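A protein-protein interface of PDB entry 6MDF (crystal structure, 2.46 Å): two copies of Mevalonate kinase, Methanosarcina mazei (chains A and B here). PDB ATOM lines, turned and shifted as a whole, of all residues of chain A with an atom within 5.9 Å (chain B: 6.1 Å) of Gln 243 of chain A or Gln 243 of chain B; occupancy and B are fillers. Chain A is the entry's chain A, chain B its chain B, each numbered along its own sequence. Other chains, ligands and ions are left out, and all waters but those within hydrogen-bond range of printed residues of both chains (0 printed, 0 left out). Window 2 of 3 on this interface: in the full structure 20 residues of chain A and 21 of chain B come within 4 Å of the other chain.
Ile 238 of chain A touches none of the printed residues of chain B.
Of the printed residues of chain B, Leu 239 of chain A touches Gln 243 and Tyr 246.
Of the printed residues of chain B, Ser 242 of chain A touches Ser 242.
Gln 243 of chain A touches just these residues of chain B: Leu 239 and Gln 243.
Printed residues of chain A within 4 Å of Leu 239 of chain B: Gln 243 (3.8 Å) and Tyr 246 (3.9 Å).
Of the printed residues of chain A, Ser 242 of chain B touches Ser 242 (2.5 Å).
Gln 243 of chain B touches just these residues of chain A: Leu 239 (3.7 Å) and Gln 243 (3.0 Å).
Leu 244 of chain B touches none of the printed residues of chain A.
The nearest printed residue of chain B that does not touch Ser 242 of chain A is Leu 239 of chain B (4.4 Å).
Printed residues of chain A that touch a printed residue of chain B: Leu 239, Ser 242, Gln 243 and Tyr 246.
Hydrophobic or aromatic side chains of chain A within 4 Å of the printed part of chain B: Leu 239 and Tyr 246.
Along chain A the printed residues that touch a printed residue of chain B span positions 239 to 246.
Printed residues of chain B that touch a printed residue of chain A: Ile 238, Leu 239, Ser 242, Gln 243 and Tyr 246.
Among the printed residues, 7 pairs touch across the chains.
Among the printed residues, no Asp or Glu carboxylate lies within 4 Å of a Lys or Arg side-chain nitrogen of the other chain.
Leu 239 of chain A touches Gln 243 of chain B, and with the chains exchanged Gln 243 of chain A touches Leu 239 of chain B.
Leu 239 of chain A touches Tyr 246 of chain B, and with the chains exchanged Tyr 246 of chain A touches Leu 239 of chain B.
Ser 242 of chain B touches its own counterpart, Ser 242 of chain A.
Gln 243 of chain B touches its own counterpart, Gln 243 of chain A.
12 positions are printed for both chains.
Of the 7 pairs that touch across the chains among the printed residues, 6 have their exchanged pair printed and touching as well.
Among the printed residues, pairs that only touch across the chains: Leu 239 of chain A with Gln 243 of chain B (3.7 Å), Leu 239 of chain A with Tyr 246 of chain B (3.8 Å), Gln 243 of chain A with Leu 239 of chain B (3.8 Å), Tyr 246 of chain A with Ile 238 of chain B (3.8 Å) and Tyr 246 of chain A with Leu 239 of chain B (3.9 Å).
OG of Ser 242 of chain A is in hydrogen-bond range of OG of Ser 242 of chain B (2.5 Å).
NE2 of Gln 243 of chain A sits at hydrogen-bond distance from OE1 of Gln 243 of chain B (3.0 Å).
The backbone carbonyl oxygen of Gln 243 of chain A is in hydrogen-bond range of the side-chain hydroxyl of Ser 247 of chain A (2.6 Å).
The backbone carbonyl oxygen (O) of Gln 243 of chain B is in hydrogen-bond range of the side-chain hydroxyl (OG) of Ser 247 of chain B (2.7 Å).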
ATOM      1  N   ILE A 238      17.057  22.806 -23.884  1.00  0.00           N
ATOM      2  CA  ILE A 238      17.010  21.921 -22.722  1.00  0.00           C
ATOM      3  C   ILE A 238      17.792  20.651 -23.035  1.00  0.00           C
ATOM      4  O   ILE A 238      18.151  20.379 -24.183  1.00  0.00           O
ATOM      5  CB  ILE A 238      15.568  21.555 -22.293  1.00  0.00           C
ATOM      6  CG1 ILE A 238      14.892  20.691 -23.360  1.00  0.00           C
ATOM      7  CG2 ILE A 238      14.749  22.803 -21.981  1.00  0.00           C
ATOM      8  CD1 ILE A 238      13.601  20.049 -22.897  1.00  0.00           C
ATOM      9  N   LEU A 239      18.036  19.865 -21.982  1.00  0.00           N
ATOM     10  CA  LEU A 239      18.827  18.641 -22.106  1.00  0.00           C
ATOM     11  C   LEU A 239      18.239  17.699 -23.152  1.00  0.00           C
ATOM     12  O   LEU A 239      18.959  17.180 -24.013  1.00  0.00           O
ATOM     13  CB  LEU A 239      18.922  17.961 -20.737  1.00  0.00           C
ATOM     14  CG  LEU A 239      19.779  16.712 -20.497  1.00  0.00           C
ATOM     15  CD1 LEU A 239      18.979  15.442 -20.740  1.00  0.00           C
ATOM     16  CD2 LEU A 239      21.030  16.725 -21.352  1.00  0.00           C
ATOM     17  N   GLU A 240      16.923  17.477 -23.100  1.00  0.00           N
ATOM     18  CA  GLU A 240      16.295  16.526 -24.012  1.00  0.00           C
ATOM     19  C   GLU A 240      16.410  16.980 -25.463  1.00  0.00           C
ATOM     20  O   GLU A 240      16.694  16.168 -26.352  1.00  0.00           O
ATOM     21  CB  GLU A 240      14.832  16.322 -23.626  1.00  0.00           C
ATOM     22  CG  GLU A 240      14.627  15.548 -22.329  1.00  0.00           C
ATOM     23  CD  GLU A 240      14.778  16.410 -21.086  1.00  0.00           C
ATOM     24  OE1 GLU A 240      14.580  15.881 -19.975  1.00  0.00           O
ATOM     25  OE2 GLU A 240      15.092  17.613 -21.213  1.00  0.00           O
ATOM     26  N   LEU A 241      16.180  18.268 -25.726  1.00  0.00           N
ATOM     27  CA  LEU A 241      16.327  18.778 -27.084  1.00  0.00           C
ATOM     28  C   LEU A 241      17.751  18.583 -27.584  1.00  0.00           C
ATOM     29  O   LEU A 241      17.972  18.123 -28.710  1.00  0.00           O
ATOM     30  CB  LEU A 241      15.938  20.256 -27.135  1.00  0.00           C
ATOM     31  CG  LEU A 241      14.455  20.607 -27.030  1.00  0.00           C
ATOM     32  CD1 LEU A 241      14.293  22.078 -26.685  1.00  0.00           C
ATOM     33  CD2 LEU A 241      13.731  20.271 -28.326  1.00  0.00           C
ATOM     34  N   SER A 242      18.732  18.920 -26.746  1.00  0.00           N
ATOM     35  CA  SER A 242      20.130  18.749 -27.125  1.00  0.00           C
ATOM     36  C   SER A 242      20.446  17.290 -27.431  1.00  0.00           C
ATOM     37  O   SER A 242      21.222  16.994 -28.348  1.00  0.00           O
ATOM     38  CB  SER A 242      21.033  19.279 -26.012  1.00  0.00           C
ATOM     39  OG  SER A 242      22.364  19.415 -26.466  1.00  0.00           O
ATOM     40  N   GLN A 243      19.843  16.362 -26.681  1.00  0.00           N
ATOM     41  CA  GLN A 243      20.110  14.944 -26.898  1.00  0.00           C
ATOM     42  C   GLN A 243      19.539  14.466 -28.226  1.00  0.00           C
ATOM     43  O   GLN A 243      20.180  13.681 -28.933  1.00  0.00           O
ATOM     44  CB  GLN A 243      19.545  14.121 -25.742  1.00  0.00           C
ATOM     45  CG  GLN A 243      20.382  14.189 -24.478  1.00  0.00           C
ATOM     46  CD  GLN A 243      19.767  13.409 -23.338  1.00  0.00           C
ATOM     47  OE1 GLN A 243      18.543  13.362 -23.195  1.00  0.00           O
ATOM     48  NE2 GLN A 243      20.612  12.788 -22.518  1.00  0.00           N
ATOM     49  N   LEU A 244      18.334  14.915 -28.579  1.00  0.00           N
ATOM     50  CA  LEU A 244      17.761  14.538 -29.868  1.00  0.00           C
ATOM     51  C   LEU A 244      18.499  15.214 -31.015  1.00  0.00           C
ATOM     52  O   LEU A 244      18.707  14.604 -32.072  1.00  0.00           O
ATOM     53  CB  LEU A 244      16.277  14.896 -29.912  1.00  0.00           C
ATOM     54  CG  LEU A 244      15.369  14.300 -28.837  1.00  0.00           C
ATOM     55  CD1 LEU A 244      13.912  14.544 -29.201  1.00  0.00           C
ATOM     56  CD2 LEU A 244      15.645  12.816 -28.656  1.00  0.00           C
ATOM     57  N   ILE A 245      18.903  16.471 -30.824  1.00  0.00           N
ATOM     58  CA  ILE A 245      19.576  17.215 -31.886  1.00  0.00           C
ATOM     59  C   ILE A 245      20.921  16.576 -32.218  1.00  0.00           C
ATOM     60  O   ILE A 245      21.244  16.344 -33.390  1.00  0.00           O
ATOM     61  CB  ILE A 245      19.732  18.691 -31.481  1.00  0.00           C
ATOM     62  CG1 ILE A 245      18.389  19.415 -31.591  1.00  0.00           C
ATOM     63  CG2 ILE A 245      20.783  19.373 -32.347  1.00  0.00           C
ATOM     64  CD1 ILE A 245      18.374  20.786 -30.952  1.00  0.00           C
ATOM     65  N   TYR A 246      21.722  16.273 -31.194  1.00  0.00           N
ATOM     66  CA  TYR A 246      23.046  15.713 -31.450  1.00  0.00           C
ATOM     67  C   TYR A 246      22.972  14.266 -31.924  1.00  0.00           C
ATOM     68  O   TYR A 246      23.805  13.839 -32.733  1.00  0.00           O
ATOM     69  CB  TYR A 246      23.924  15.835 -30.205  1.00  0.00           C
ATOM     70  CG  TYR A 246      24.687  17.136 -30.179  1.00  0.00           C
ATOM     71  CD1 TYR A 246      25.823  17.310 -30.958  1.00  0.00           C
ATOM     72  CD2 TYR A 246      24.257  18.203 -29.401  1.00  0.00           C
ATOM     73  CE1 TYR A 246      26.516  18.504 -30.954  1.00  0.00           C
ATOM     74  CE2 TYR A 246      24.945  19.402 -29.389  1.00  0.00           C
ATOM     75  CZ  TYR A 246      26.076  19.546 -30.168  1.00  0.00           C
ATOM     76  OH  TYR A 246      26.767  20.738 -30.165  1.00  0.00           O
ATOM     77  N   SER A 247      21.981  13.503 -31.454  1.00  0.00           N
ATOM     78  CA  SER A 247      21.785  12.156 -31.976  1.00  0.00           C
ATOM     79  C   SER A 247      21.473  12.188 -33.466  1.00  0.00           C
ATOM     80  O   SER A 247      21.960  11.344 -34.229  1.00  0.00           O
ATOM     81  CB  SER A 247      20.667  11.447 -31.211  1.00  0.00           C
ATOM     82  OG  SER A 247      20.959  11.369 -29.824  1.00  0.00           O
ATOM     83  N   ALA A 248      20.669  13.162 -33.901  1.00  0.00           N
ATOM     84  CA  ALA A 248      20.321  13.254 -35.314  1.00  0.00           C
ATOM     85  C   ALA A 248      21.533  13.631 -36.155  1.00  0.00           C
ATOM     86  O   ALA A 248      21.755  13.052 -37.224  1.00  0.00           O
ATOM     87  CB  ALA A 248      19.190  14.262 -35.515  1.00  0.00           C
ATOM     88  N   ALA A 286      17.417   7.996 -28.625  1.00  0.00           N
ATOM     89  CA  ALA A 286      17.745   9.000 -27.622  1.00  0.00           C
ATOM     90  C   ALA A 286      16.540   9.403 -26.787  1.00  0.00           C
ATOM     91  O   ALA A 286      16.636  10.350 -26.000  1.00  0.00           O
ATOM     92  CB  ALA A 286      18.353  10.236 -28.287  1.00  0.00           C
ATOM     93  N   ILE B 238      29.673  19.031 -28.166  1.00  0.00           N
ATOM     94  CA  ILE B 238      29.269  17.673 -28.508  1.00  0.00           C
ATOM     95  C   ILE B 238      28.202  17.219 -27.519  1.00  0.00           C
ATOM     96  O   ILE B 238      27.884  17.914 -26.552  1.00  0.00           O
ATOM     97  CB  ILE B 238      30.453  16.682 -28.518  1.00  0.00           C
ATOM     98  CG1 ILE B 238      30.981  16.454 -27.100  1.00  0.00           C
ATOM     99  CG2 ILE B 238      31.566  17.157 -29.448  1.00  0.00           C
ATOM    100  CD1 ILE B 238      32.052  15.392 -27.023  1.00  0.00           C
ATOM    101  N   LEU B 239      27.659  16.025 -27.770  1.00  0.00           N
ATOM    102  CA  LEU B 239      26.573  15.496 -26.949  1.00  0.00           C
ATOM    103  C   LEU B 239      26.994  15.348 -25.493  1.00  0.00           C
ATOM    104  O   LEU B 239      26.264  15.744 -24.579  1.00  0.00           O
ATOM    105  CB  LEU B 239      26.111  14.149 -27.507  1.00  0.00           C
ATOM    106  CG  LEU B 239      25.191  13.322 -26.605  1.00  0.00           C
ATOM    107  CD1 LEU B 239      23.803  13.940 -26.545  1.00  0.00           C
ATOM    108  CD2 LEU B 239      25.121  11.877 -27.075  1.00  0.00           C
ATOM    109  N   GLU B 240      28.173  14.773 -25.259  1.00  0.00           N
ATOM    110  CA  GLU B 240      28.597  14.486 -23.893  1.00  0.00           C
ATOM    111  C   GLU B 240      28.795  15.767 -23.094  1.00  0.00           C
ATOM    112  O   GLU B 240      28.383  15.850 -21.931  1.00  0.00           O
ATOM    113  CB  GLU B 240      29.876  13.648 -23.910  1.00  0.00           C
ATOM    114  CG  GLU B 240      29.667  12.209 -24.362  1.00  0.00           C
ATOM    115  CD  GLU B 240      29.786  12.030 -25.865  1.00  0.00           C
ATOM    116  OE1 GLU B 240      29.710  13.030 -26.609  1.00  0.00           O
ATOM    117  OE2 GLU B 240      29.964  10.879 -26.306  1.00  0.00           O
ATOM    118  N   LEU B 241      29.416  16.782 -23.702  1.00  0.00           N
ATOM    119  CA  LEU B 241      29.562  18.065 -23.024  1.00  0.00           C
ATOM    120  C   LEU B 241      28.203  18.666 -22.695  1.00  0.00           C
ATOM    121  O   LEU B 241      27.996  19.189 -21.595  1.00  0.00           O
ATOM    122  CB  LEU B 241      30.369  19.033 -23.887  1.00  0.00           C
ATOM    123  CG  LEU B 241      31.865  18.780 -24.069  1.00  0.00           C
ATOM    124  CD1 LEU B 241      32.377  19.530 -25.287  1.00  0.00           C
ATOM    125  CD2 LEU B 241      32.629  19.193 -22.824  1.00  0.00           C
ATOM    126  N   SER B 242      27.260  18.591 -23.634  1.00  0.00           N
ATOM    127  CA  SER B 242      25.951  19.195 -23.415  1.00  0.00           C
ATOM    128  C   SER B 242      25.190  18.488 -22.299  1.00  0.00           C
ATOM    129  O   SER B 242      24.469  19.133 -21.528  1.00  0.00           O
ATOM    130  CB  SER B 242      25.147  19.180 -24.716  1.00  0.00           C
ATOM    131  OG  SER B 242      24.001  20.002 -24.610  1.00  0.00           O
ATOM    132  N   GLN B 243      25.341  17.165 -22.192  1.00  0.00           N
ATOM    133  CA  GLN B 243      24.665  16.422 -21.133  1.00  0.00           C
ATOM    134  C   GLN B 243      25.210  16.794 -19.759  1.00  0.00           C
ATOM    135  O   GLN B 243      24.441  16.965 -18.805  1.00  0.00           O
ATOM    136  CB  GLN B 243      24.807  14.920 -21.377  1.00  0.00           C
ATOM    137  CG  GLN B 243      24.007  14.411 -22.560  1.00  0.00           C
ATOM    138  CD  GLN B 243      24.324  12.968 -22.902  1.00  0.00           C
ATOM    139  OE1 GLN B 243      23.450  12.214 -23.329  1.00  0.00           O
ATOM    140  NE2 GLN B 243      25.581  12.578 -22.722  1.00  0.00           N
ATOM    141  N   LEU B 244      26.533  16.920 -19.637  1.00  0.00           N
ATOM    142  CA  LEU B 244      27.114  17.312 -18.357  1.00  0.00           C
ATOM    143  C   LEU B 244      26.745  18.746 -18.005  1.00  0.00           C
ATOM    144  O   LEU B 244      26.466  19.057 -16.842  1.00  0.00           O
ATOM    145  CB  LEU B 244      28.633  17.144 -18.397  1.00  0.00           C
ATOM    146  CG  LEU B 244      29.195  15.783 -18.822  1.00  0.00           C
ATOM    147  CD1 LEU B 244      30.677  15.687 -18.478  1.00  0.00           C
ATOM    148  CD2 LEU B 244      28.415  14.628 -18.197  1.00  0.00           C
ATOM    149  N   ILE B 245      26.728  19.630 -19.005  1.00  0.00           N
ATOM    150  CA  ILE B 245      26.422  21.037 -18.763  1.00  0.00           C
ATOM    151  C   ILE B 245      24.996  21.193 -18.246  1.00  0.00           C
ATOM    152  O   ILE B 245      24.749  21.880 -17.247  1.00  0.00           O
ATOM    153  CB  ILE B 245      26.660  21.854 -20.045  1.00  0.00           C
ATOM    154  CG1 ILE B 245      28.162  22.042 -20.272  1.00  0.00           C
ATOM    155  CG2 ILE B 245      25.951  23.198 -19.979  1.00  0.00           C
ATOM    156  CD1 ILE B 245      28.514  22.547 -21.647  1.00  0.00           C
ATOM    157  N   TYR B 246      24.035  20.544 -18.905  1.00  0.00           N
ATOM    158  CA  TYR B 246      22.643  20.741 -18.518  1.00  0.00           C
ATOM    159  C   TYR B 246      22.307  20.024 -17.217  1.00  0.00           C
ATOM    160  O   TYR B 246      21.426  20.475 -16.477  1.00  0.00           O
ATOM    161  CB  TYR B 246      21.716  20.302 -19.653  1.00  0.00           C
ATOM    162  CG  TYR B 246      21.546  21.396 -20.679  1.00  0.00           C
ATOM    163  CD1 TYR B 246      20.726  22.490 -20.422  1.00  0.00           C
ATOM    164  CD2 TYR B 246      22.233  21.359 -21.888  1.00  0.00           C
ATOM    165  CE1 TYR B 246      20.581  23.508 -21.346  1.00  0.00           C
ATOM    166  CE2 TYR B 246      22.093  22.374 -22.820  1.00  0.00           C
ATOM    167  CZ  TYR B 246      21.266  23.446 -22.543  1.00  0.00           C
ATOM    168  OH  TYR B 246      21.123  24.458 -23.465  1.00  0.00           O
ATOM    169  N   SER B 247      23.001  18.923 -16.913  1.00  0.00           N
ATOM    170  CA  SER B 247      22.794  18.265 -15.627  1.00  0.00           C
ATOM    171  C   SER B 247      23.278  19.140 -14.480  1.00  0.00           C
ATOM    172  O   SER B 247      22.649  19.184 -13.417  1.00  0.00           O
ATOM    173  CB  SER B 247      23.502  16.914 -15.606  1.00  0.00           C
ATOM    174  OG  SER B 247      23.016  16.095 -16.656  1.00  0.00           O
ATOM    175  N   ALA B 248      24.389  19.850 -14.683  1.00  0.00           N
ATOM    176  CA  ALA B 248      24.870  20.779 -13.667  1.00  0.00           C
ATOM    177  C   ALA B 248      23.892  21.930 -13.465  1.00  0.00           C
ATOM    178  O   ALA B 248      23.611  22.319 -12.324  1.00  0.00           O
ATOM    179  CB  ALA B 248      26.249  21.308 -14.052  1.00  0.00           C
ATOM    180  N   ALA B 286      25.311  12.009 -14.733  1.00  0.00           N
ATOM    181  CA  ALA B 286      25.171  12.163 -16.174  1.00  0.00           C
ATOM    182  C   ALA B 286      26.313  11.521 -16.949  1.00  0.00           C
ATOM    183  O   ALA B 286      26.300  11.557 -18.185  1.00  0.00           O
ATOM    184  CB  ALA B 286      25.071  13.647 -16.539  1.00  0.00           C
